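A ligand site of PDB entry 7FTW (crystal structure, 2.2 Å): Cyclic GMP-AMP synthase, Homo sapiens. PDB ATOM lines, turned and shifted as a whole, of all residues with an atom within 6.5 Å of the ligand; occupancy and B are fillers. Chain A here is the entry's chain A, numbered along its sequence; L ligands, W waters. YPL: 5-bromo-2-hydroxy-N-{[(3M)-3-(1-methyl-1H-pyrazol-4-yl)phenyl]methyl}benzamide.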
ATOM      1  N   ALA A  87       6.777  -3.495 -15.703  1.00  0.00           N
ATOM      2  CA  ALA A  87       7.141  -3.795 -17.083  1.00  0.00           C
ATOM      3  C   ALA A  87       6.555  -2.855 -18.126  1.00  0.00           C
ATOM      4  O   ALA A  87       7.000  -2.888 -19.277  1.00  0.00           O
ATOM      5  CB  ALA A  87       6.728  -5.238 -17.434  1.00  0.00           C
ATOM      6  N   TYR A  88       5.574  -2.036 -17.776  1.00  0.00           N
ATOM      7  CA  TYR A  88       4.978  -1.098 -18.720  1.00  0.00           C
ATOM      8  C   TYR A  88       5.291   0.329 -18.287  1.00  0.00           C
ATOM      9  O   TYR A  88       5.267   0.649 -17.097  1.00  0.00           O
ATOM     10  CB  TYR A  88       3.479  -1.370 -18.824  1.00  0.00           C
ATOM     11  CG  TYR A  88       3.158  -2.748 -19.394  1.00  0.00           C
ATOM     12  CD1 TYR A  88       3.182  -2.983 -20.768  1.00  0.00           C
ATOM     13  CD2 TYR A  88       2.822  -3.816 -18.570  1.00  0.00           C
ATOM     14  CE1 TYR A  88       2.888  -4.226 -21.311  1.00  0.00           C
ATOM     15  CE2 TYR A  88       2.519  -5.080 -19.108  1.00  0.00           C
ATOM     16  CZ  TYR A  88       2.562  -5.265 -20.471  1.00  0.00           C
ATOM     17  OH  TYR A  88       2.271  -6.503 -21.027  1.00  0.00           O
ATOM     18  N   HIS A 203      -0.206  -3.960 -26.427  1.00  0.00           N
ATOM     19  CA  HIS A 203      -1.331  -4.353 -27.285  1.00  0.00           C
ATOM     20  C   HIS A 203      -2.545  -4.771 -26.473  1.00  0.00           C
ATOM     21  O   HIS A 203      -3.491  -3.992 -26.300  1.00  0.00           O
ATOM     22  CB  HIS A 203      -0.909  -5.482 -28.242  1.00  0.00           C
ATOM     23  CG  HIS A 203      -0.170  -6.624 -27.597  1.00  0.00           C
ATOM     24  ND1 HIS A 203       0.809  -6.443 -26.647  1.00  0.00           N
ATOM     25  CD2 HIS A 203      -0.245  -7.959 -27.804  1.00  0.00           C
ATOM     26  CE1 HIS A 203       1.284  -7.625 -26.281  1.00  0.00           C
ATOM     27  NE2 HIS A 203       0.659  -8.552 -26.971  1.00  0.00           N
ATOM     28  N   ARG A 216       6.335  -1.365 -23.389  1.00  0.00           N
ATOM     29  CA  ARG A 216       7.123  -2.348 -22.636  1.00  0.00           C
ATOM     30  C   ARG A 216       8.448  -2.598 -23.320  1.00  0.00           C
ATOM     31  O   ARG A 216       8.638  -2.293 -24.504  1.00  0.00           O
ATOM     32  CB  ARG A 216       6.383  -3.686 -22.428  1.00  0.00           C
ATOM     33  CG  ARG A 216       5.814  -4.346 -23.651  1.00  0.00           C
ATOM     34  CD  ARG A 216       6.744  -5.390 -24.188  1.00  0.00           C
ATOM     35  NE  ARG A 216       6.211  -6.118 -25.346  1.00  0.00           N
ATOM     36  CZ  ARG A 216       6.949  -6.930 -26.100  1.00  0.00           C
ATOM     37  NH1 ARG A 216       8.241  -7.093 -25.807  1.00  0.00           N
ATOM     38  NH2 ARG A 216       6.409  -7.563 -27.138  1.00  0.00           N
ATOM     39  N   LEU A 217       9.363  -3.196 -22.551  1.00  0.00           N
ATOM     40  CA  LEU A 217      10.716  -3.485 -23.001  1.00  0.00           C
ATOM     41  C   LEU A 217      10.737  -4.688 -23.936  1.00  0.00           C
ATOM     42  O   LEU A 217      10.010  -5.669 -23.737  1.00  0.00           O
ATOM     43  CB  LEU A 217      11.617  -3.772 -21.807  1.00  0.00           C
ATOM     44  CG  LEU A 217      12.053  -2.605 -20.932  1.00  0.00           C
ATOM     45  CD1 LEU A 217      12.180  -3.000 -19.477  1.00  0.00           C
ATOM     46  CD2 LEU A 217      13.375  -2.179 -21.460  1.00  0.00           C
ATOM     47  N   SER A 218      11.606  -4.626 -24.936  1.00  0.00           N
ATOM     48  CA  SER A 218      11.850  -5.723 -25.865  1.00  0.00           C
ATOM     49  C   SER A 218      13.324  -6.112 -25.776  1.00  0.00           C
ATOM     50  O   SER A 218      14.200  -5.245 -25.833  1.00  0.00           O
ATOM     51  CB  SER A 218      11.465  -5.342 -27.308  1.00  0.00           C
ATOM     52  OG  SER A 218      11.914  -6.294 -28.267  1.00  0.00           O
ATOM     53  N   PHE A 219      13.582  -7.409 -25.616  1.00  0.00           N
ATOM     54  CA  PHE A 219      14.935  -7.942 -25.462  1.00  0.00           C
ATOM     55  C   PHE A 219      15.231  -9.023 -26.491  1.00  0.00           C
ATOM     56  O   PHE A 219      16.100  -9.885 -26.283  1.00  0.00           O
ATOM     57  CB  PHE A 219      15.137  -8.470 -24.050  1.00  0.00           C
ATOM     58  CG  PHE A 219      15.160  -7.409 -22.994  1.00  0.00           C
ATOM     59  CD1 PHE A 219      16.280  -6.633 -22.821  1.00  0.00           C
ATOM     60  CD2 PHE A 219      14.083  -7.223 -22.145  1.00  0.00           C
ATOM     61  CE1 PHE A 219      16.326  -5.647 -21.819  1.00  0.00           C
ATOM     62  CE2 PHE A 219      14.120  -6.239 -21.146  1.00  0.00           C
ATOM     63  CZ  PHE A 219      15.247  -5.461 -20.993  1.00  0.00           C
ATOM     64  N   SER A 220      14.512  -8.997 -27.611  1.00  0.00           N
ATOM     65  CA  SER A 220      14.741  -9.949 -28.684  1.00  0.00           C
ATOM     66  C   SER A 220      16.192  -9.965 -29.121  1.00  0.00           C
ATOM     67  O   SER A 220      16.726 -11.013 -29.499  1.00  0.00           O
ATOM     68  CB  SER A 220      13.840  -9.617 -29.874  1.00  0.00           C
ATOM     69  OG  SER A 220      12.540 -10.146 -29.666  1.00  0.00           O
ATOM     70  N   HIS A 221      16.859  -8.810 -29.056  1.00  0.00           N
ATOM     71  CA  HIS A 221      18.254  -8.771 -29.458  1.00  0.00           C
ATOM     72  C   HIS A 221      19.141  -9.444 -28.427  1.00  0.00           C
ATOM     73  O   HIS A 221      20.187 -10.000 -28.785  1.00  0.00           O
ATOM     74  CB  HIS A 221      18.712  -7.332 -29.662  1.00  0.00           C
ATOM     75  CG  HIS A 221      18.667  -6.501 -28.417  1.00  0.00           C
ATOM     76  ND1 HIS A 221      17.540  -6.379 -27.633  1.00  0.00           N
ATOM     77  CD2 HIS A 221      19.610  -5.711 -27.850  1.00  0.00           C
ATOM     78  CE1 HIS A 221      17.793  -5.553 -26.631  1.00  0.00           C
ATOM     79  NE2 HIS A 221      19.053  -5.147 -26.737  1.00  0.00           N
ATOM     80  N   GLU A 223      18.123 -12.031 -26.423  1.00  0.00           N
ATOM     81  CA  GLU A 223      17.804 -13.402 -26.775  1.00  0.00           C
ATOM     82  C   GLU A 223      18.678 -13.926 -27.899  1.00  0.00           C
ATOM     83  O   GLU A 223      19.361 -14.943 -27.742  1.00  0.00           O
ATOM     84  CB  GLU A 223      16.326 -13.507 -27.179  1.00  0.00           C
ATOM     85  CG  GLU A 223      15.960 -14.870 -27.786  1.00  0.00           C
ATOM     86  CD  GLU A 223      14.618 -14.881 -28.528  1.00  0.00           C
ATOM     87  OE1 GLU A 223      14.280 -15.925 -29.133  1.00  0.00           O
ATOM     88  OE2 GLU A 223      13.891 -13.871 -28.516  1.00  0.00           O
ATOM     89  N   SER A 274       2.172 -17.356 -26.134  1.00  0.00           N
ATOM     90  CA  SER A 274       3.043 -17.163 -27.288  1.00  0.00           C
ATOM     91  C   SER A 274       4.410 -17.798 -27.042  1.00  0.00           C
ATOM     92  O   SER A 274       4.728 -18.242 -25.937  1.00  0.00           O
ATOM     93  CB  SER A 274       3.221 -15.693 -27.575  1.00  0.00           C
ATOM     94  OG  SER A 274       3.894 -15.105 -26.488  1.00  0.00           O
ATOM     95  N   TYR A 276       6.962 -16.354 -26.591  1.00  0.00           N
ATOM     96  CA  TYR A 276       7.581 -15.608 -25.508  1.00  0.00           C
ATOM     97  C   TYR A 276       7.442 -16.343 -24.167  1.00  0.00           C
ATOM     98  O   TYR A 276       8.365 -16.353 -23.350  1.00  0.00           O
ATOM     99  CB  TYR A 276       6.956 -14.213 -25.502  1.00  0.00           C
ATOM    100  CG  TYR A 276       6.843 -13.495 -24.206  1.00  0.00           C
ATOM    101  CD1 TYR A 276       7.974 -12.954 -23.589  1.00  0.00           C
ATOM    102  CD2 TYR A 276       5.590 -13.247 -23.640  1.00  0.00           C
ATOM    103  CE1 TYR A 276       7.862 -12.254 -22.413  1.00  0.00           C
ATOM    104  CE2 TYR A 276       5.468 -12.540 -22.471  1.00  0.00           C
ATOM    105  CZ  TYR A 276       6.609 -12.052 -21.851  1.00  0.00           C
ATOM    106  OH  TYR A 276       6.495 -11.333 -20.683  1.00  0.00           O
ATOM    107  N   HIS A 277       6.316 -17.004 -23.915  1.00  0.00           N
ATOM    108  CA  HIS A 277       6.217 -17.768 -22.674  1.00  0.00           C
ATOM    109  C   HIS A 277       7.158 -18.962 -22.696  1.00  0.00           C
ATOM    110  O   HIS A 277       7.684 -19.365 -21.659  1.00  0.00           O
ATOM    111  CB  HIS A 277       4.787 -18.225 -22.480  1.00  0.00           C
ATOM    112  CG  HIS A 277       3.833 -17.087 -22.383  1.00  0.00           C
ATOM    113  ND1 HIS A 277       3.090 -16.663 -23.462  1.00  0.00           N
ATOM    114  CD2 HIS A 277       3.560 -16.248 -21.364  1.00  0.00           C
ATOM    115  CE1 HIS A 277       2.375 -15.610 -23.093  1.00  0.00           C
ATOM    116  NE2 HIS A 277       2.639 -15.338 -21.832  1.00  0.00           N
ATOM    117  N   LYS A 279      10.089 -19.326 -24.638  1.00  0.00           N
ATOM    118  CA  LYS A 279      11.476 -18.849 -24.523  1.00  0.00           C
ATOM    119  C   LYS A 279      11.807 -18.509 -23.088  1.00  0.00           C
ATOM    120  O   LYS A 279      12.895 -18.822 -22.602  1.00  0.00           O
ATOM    121  CB  LYS A 279      11.714 -17.619 -25.383  1.00  0.00           C
ATOM    122  CG  LYS A 279      11.472 -17.745 -26.865  1.00  0.00           C
ATOM    123  CD  LYS A 279      11.576 -16.330 -27.474  1.00  0.00           C
ATOM    124  CE  LYS A 279      11.208 -16.287 -28.948  1.00  0.00           C
ATOM    125  NZ  LYS A 279      11.117 -14.860 -29.367  1.00  0.00           N
ATOM    126  N   THR A 280      10.872 -17.844 -22.392  1.00  0.00           N
ATOM    127  CA  THR A 280      11.153 -17.416 -21.025  1.00  0.00           C
ATOM    128  C   THR A 280      11.383 -18.611 -20.109  1.00  0.00           C
ATOM    129  O   THR A 280      12.370 -18.667 -19.386  1.00  0.00           O
ATOM    130  CB  THR A 280      10.014 -16.534 -20.500  1.00  0.00           C
ATOM    131  OG1 THR A 280      10.052 -15.279 -21.165  1.00  0.00           O
ATOM    132  CG2 THR A 280      10.187 -16.300 -19.008  1.00  0.00           C
ATOM    133  N   PHE A 283      14.776 -20.271 -20.826  1.00  0.00           N
ATOM    134  CA  PHE A 283      15.981 -19.660 -20.286  1.00  0.00           C
ATOM    135  C   PHE A 283      16.113 -19.931 -18.797  1.00  0.00           C
ATOM    136  O   PHE A 283      17.226 -20.046 -18.285  1.00  0.00           O
ATOM    137  CB  PHE A 283      15.992 -18.159 -20.575  1.00  0.00           C
ATOM    138  CG  PHE A 283      16.384 -17.821 -21.998  1.00  0.00           C
ATOM    139  CD1 PHE A 283      17.363 -18.543 -22.631  1.00  0.00           C
ATOM    140  CD2 PHE A 283      15.755 -16.813 -22.695  1.00  0.00           C
ATOM    141  CE1 PHE A 283      17.722 -18.253 -23.956  1.00  0.00           C
ATOM    142  CE2 PHE A 283      16.109 -16.511 -24.016  1.00  0.00           C
ATOM    143  CZ  PHE A 283      17.075 -17.231 -24.643  1.00  0.00           C
ATOM    144  N   ASN A 322       9.307 -13.154 -15.590  1.00  0.00           N
ATOM    145  CA  ASN A 322       9.993 -12.632 -16.756  1.00  0.00           C
ATOM    146  C   ASN A 322      11.490 -12.790 -16.563  1.00  0.00           C
ATOM    147  O   ASN A 322      12.007 -12.554 -15.459  1.00  0.00           O
ATOM    148  CB  ASN A 322       9.633 -11.169 -16.942  1.00  0.00           C
ATOM    149  CG  ASN A 322      10.272 -10.568 -18.147  1.00  0.00           C
ATOM    150  OD1 ASN A 322      11.466 -10.264 -18.149  1.00  0.00           O
ATOM    151  ND2 ASN A 322       9.486 -10.358 -19.183  1.00  0.00           N
ATOM    152  N   TYR A 323      12.189 -13.200 -17.620  1.00  0.00           N
ATOM    153  CA  TYR A 323      13.619 -13.499 -17.491  1.00  0.00           C
ATOM    154  C   TYR A 323      14.439 -12.228 -17.282  1.00  0.00           C
ATOM    155  O   TYR A 323      15.547 -12.301 -16.720  1.00  0.00           O
ATOM    156  CB  TYR A 323      14.111 -14.280 -18.719  1.00  0.00           C
ATOM    157  CG  TYR A 323      15.441 -15.005 -18.499  1.00  0.00           C
ATOM    158  CD1 TYR A 323      15.522 -16.098 -17.652  1.00  0.00           C
ATOM    159  CD2 TYR A 323      16.604 -14.561 -19.111  1.00  0.00           C
ATOM    160  CE1 TYR A 323      16.716 -16.753 -17.424  1.00  0.00           C
ATOM    161  CE2 TYR A 323      17.811 -15.217 -18.889  1.00  0.00           C
ATOM    162  CZ  TYR A 323      17.856 -16.300 -18.038  1.00  0.00           C
ATOM    163  OH  TYR A 323      19.055 -16.941 -17.802  1.00  0.00           O
ATOM    164  N   PHE A 324      13.912 -11.071 -17.672  1.00  0.00           N
ATOM    165  CA  PHE A 324      14.648  -9.821 -17.523  1.00  0.00           C
ATOM    166  C   PHE A 324      14.129  -8.988 -16.373  1.00  0.00           C
ATOM    167  O   PHE A 324      14.861  -8.121 -15.868  1.00  0.00           O
ATOM    168  CB  PHE A 324      14.560  -8.997 -18.821  1.00  0.00           C
ATOM    169  CG  PHE A 324      15.191  -9.685 -19.981  1.00  0.00           C
ATOM    170  CD1 PHE A 324      14.511 -10.676 -20.658  1.00  0.00           C
ATOM    171  CD2 PHE A 324      16.488  -9.380 -20.355  1.00  0.00           C
ATOM    172  CE1 PHE A 324      15.097 -11.374 -21.706  1.00  0.00           C
ATOM    173  CE2 PHE A 324      17.086 -10.079 -21.409  1.00  0.00           C
ATOM    174  CZ  PHE A 324      16.381 -11.077 -22.071  1.00  0.00           C
ATOM    175  N   ILE A 325      12.908  -9.265 -15.921  1.00  0.00           N
ATOM    176  CA  ILE A 325      12.210  -8.415 -14.957  1.00  0.00           C
ATOM    177  C   ILE A 325      11.674  -9.346 -13.879  1.00  0.00           C
ATOM    178  O   ILE A 325      10.522  -9.797 -13.974  1.00  0.00           O
ATOM    179  CB  ILE A 325      11.105  -7.603 -15.649  1.00  0.00           C
ATOM    180  CG1 ILE A 325      11.697  -6.793 -16.817  1.00  0.00           C
ATOM    181  CG2 ILE A 325      10.389  -6.693 -14.669  1.00  0.00           C
ATOM    182  CD1 ILE A 325      10.668  -6.326 -17.871  1.00  0.00           C
ATOM    183  N   PHE A 328       7.823  -9.543 -12.562  1.00  0.00           N
ATOM    184  CA  PHE A 328       6.694  -9.553 -13.492  1.00  0.00           C
ATOM    185  C   PHE A 328       6.352 -11.004 -13.823  1.00  0.00           C
ATOM    186  O   PHE A 328       7.146 -11.717 -14.455  1.00  0.00           O
ATOM    187  CB  PHE A 328       7.064  -8.755 -14.726  1.00  0.00           C
ATOM    188  CG  PHE A 328       6.011  -8.734 -15.775  1.00  0.00           C
ATOM    189  CD1 PHE A 328       4.734  -8.325 -15.467  1.00  0.00           C
ATOM    190  CD2 PHE A 328       6.307  -9.057 -17.069  1.00  0.00           C
ATOM    191  CE1 PHE A 328       3.760  -8.288 -16.443  1.00  0.00           C
ATOM    192  CE2 PHE A 328       5.325  -9.022 -18.048  1.00  0.00           C
ATOM    193  CZ  PHE A 328       4.045  -8.628 -17.724  1.00  0.00           C
ATOM    194  N   LEU A 330       4.417 -13.653 -15.800  1.00  0.00           N
ATOM    195  CA  LEU A 330       3.679 -13.827 -17.055  1.00  0.00           C
ATOM    196  C   LEU A 330       2.438 -14.681 -16.880  1.00  0.00           C
ATOM    197  O   LEU A 330       1.537 -14.628 -17.728  1.00  0.00           O
ATOM    198  CB  LEU A 330       4.553 -14.472 -18.131  1.00  0.00           C
ATOM    199  CG  LEU A 330       6.017 -14.062 -18.235  1.00  0.00           C
ATOM    200  CD1 LEU A 330       6.595 -14.531 -19.538  1.00  0.00           C
ATOM    201  CD2 LEU A 330       6.187 -12.570 -18.061  1.00  0.00           C
HETATM  202  C10 YPL L   1       5.478  -7.951 -21.904  1.00  0.00           C
HETATM  203  C11 YPL L   1       6.195  -8.655 -22.860  1.00  0.00           C
HETATM  204  C13 YPL L   1       5.495  -9.374 -23.942  1.00  0.00           C
HETATM  205  C17 YPL L   1       4.101  -9.440 -24.142  1.00  0.00           C
HETATM  206  C18 YPL L   1       4.968 -11.417 -26.886  1.00  0.00           C
HETATM  207  C20 YPL L   1      12.018 -12.079 -23.246  1.00  0.00           C
HETATM  208  C21 YPL L   1      12.618 -12.803 -24.255  1.00  0.00           C
HETATM  209  C23 YPL L   1      12.761 -12.299 -25.526  1.00  0.00           C
HETATM  210  C24 YPL L   1      12.289 -11.032 -25.797  1.00  0.00           C
HETATM  211  C12 YPL L   1       7.595  -8.675 -22.786  1.00  0.00           C
HETATM  212  C14 YPL L   1       5.984 -10.140 -24.981  1.00  0.00           C
HETATM  213  C2  YPL L   1      11.677 -10.265 -24.811  1.00  0.00           C
HETATM  214  C3  YPL L   1      11.533 -10.802 -23.516  1.00  0.00           C
HETATM  215  C4  YPL L   1      10.889 -10.028 -22.407  1.00  0.00           C
HETATM  216  C6  YPL L   1       9.767  -7.999 -21.671  1.00  0.00           C
HETATM  217  C7  YPL L   1       8.248  -7.987 -21.769  1.00  0.00           C
HETATM  218  C8  YPL L   1       7.506  -7.293 -20.831  1.00  0.00           C
HETATM  219  C9  YPL L   1       6.125  -7.269 -20.899  1.00  0.00           C
HETATM  220  N15 YPL L   1       4.940 -10.584 -25.692  1.00  0.00           N
HETATM  221  N16 YPL L   1       3.762 -10.156 -25.177  1.00  0.00           N
HETATM  222  N5  YPL L   1      10.427  -8.805 -22.680  1.00  0.00           N
HETATM  223  O1  YPL L   1      11.232  -9.041 -25.135  1.00  0.00           O
HETATM  224  O19 YPL L   1      10.773 -10.520 -21.292  1.00  0.00           O
HETATM  225 BR22 YPL L   1      13.293 -14.541 -23.874  1.00  0.00          BR
HETATM  226  O   HOH W   1      11.057 -13.113 -20.216  1.00  0.00           O
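The side-chain amide nitrogen (ND2) of Asn 322 is in hydrogen-bond range of the side-chain hydroxyl (OH) of Tyr 276, 3.5 Å away. The backbone carbonyl oxygen (O) of Phe 328 lies within hydrogen-bond range of the backbone NH (N) of Asn 322. N of Phe 324 lies within hydrogen-bond range of OD1 of Asn 322 (2.6 Å). OD1 of Asn 322 is in hydrogen-bond range of N of Ile 325. The backbone NH (N) of Tyr 276 lies close to the side-chain hydroxyl (OG) of Ser 274. O of Tyr 276 is in hydrogen-bond range of OG1 of Thr 280, 3.0 Å away. NZ of Lys 279 lies within salt-bridge range of OE2 of Glu 223 (3.1 Å). The backbone NH of Ser 274 sits at hydrogen-bond distance from a ring nitrogen (ND1) of His 277 (2.9 Å).
Residues that only touch the ligand: Arg 216 (3.4 Å), Tyr 276 (3.4 Å), Phe 283 (3.4 Å), Phe 328 (3.4 Å), Ser 218 (3.5 Å), Phe 324 (3.5 Å), Ser 220 (3.5 Å), Glu 223 (3.6 Å), Tyr 88 (3.6 Å), His 203 (3.7 Å), Lys 279 (3.8 Å) and Ser 274 (3.9 Å). Hydrophobic or aromatic side chains that line the ligand: His 203, Phe 219, Tyr 276, Phe 283, Phe 324 and Phe 328. Of the 22 residues printed, 15 come within 4 Å of the ligand. The nearest printed residue that does not touch the ligand is Ala 87 (4.05 Å).
Water W1 lies within hydrogen-bond range of OG1 of Thr 280, O19 of the ligand, N of Tyr 323 and ND2 of Asn 322.
O19 of the ligand sits at hydrogen-bond distance from ND2 of Asn 322 (2.5 Å). The backbone NH (N) of Phe 219 lies within hydrogen-bond range of an oxygen (O1) of the ligand (2.9 Å). The backbone carbonyl oxygen (O) of Leu 217 sits close to a nitrogen (N5) of the ligand (3.3 Å).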
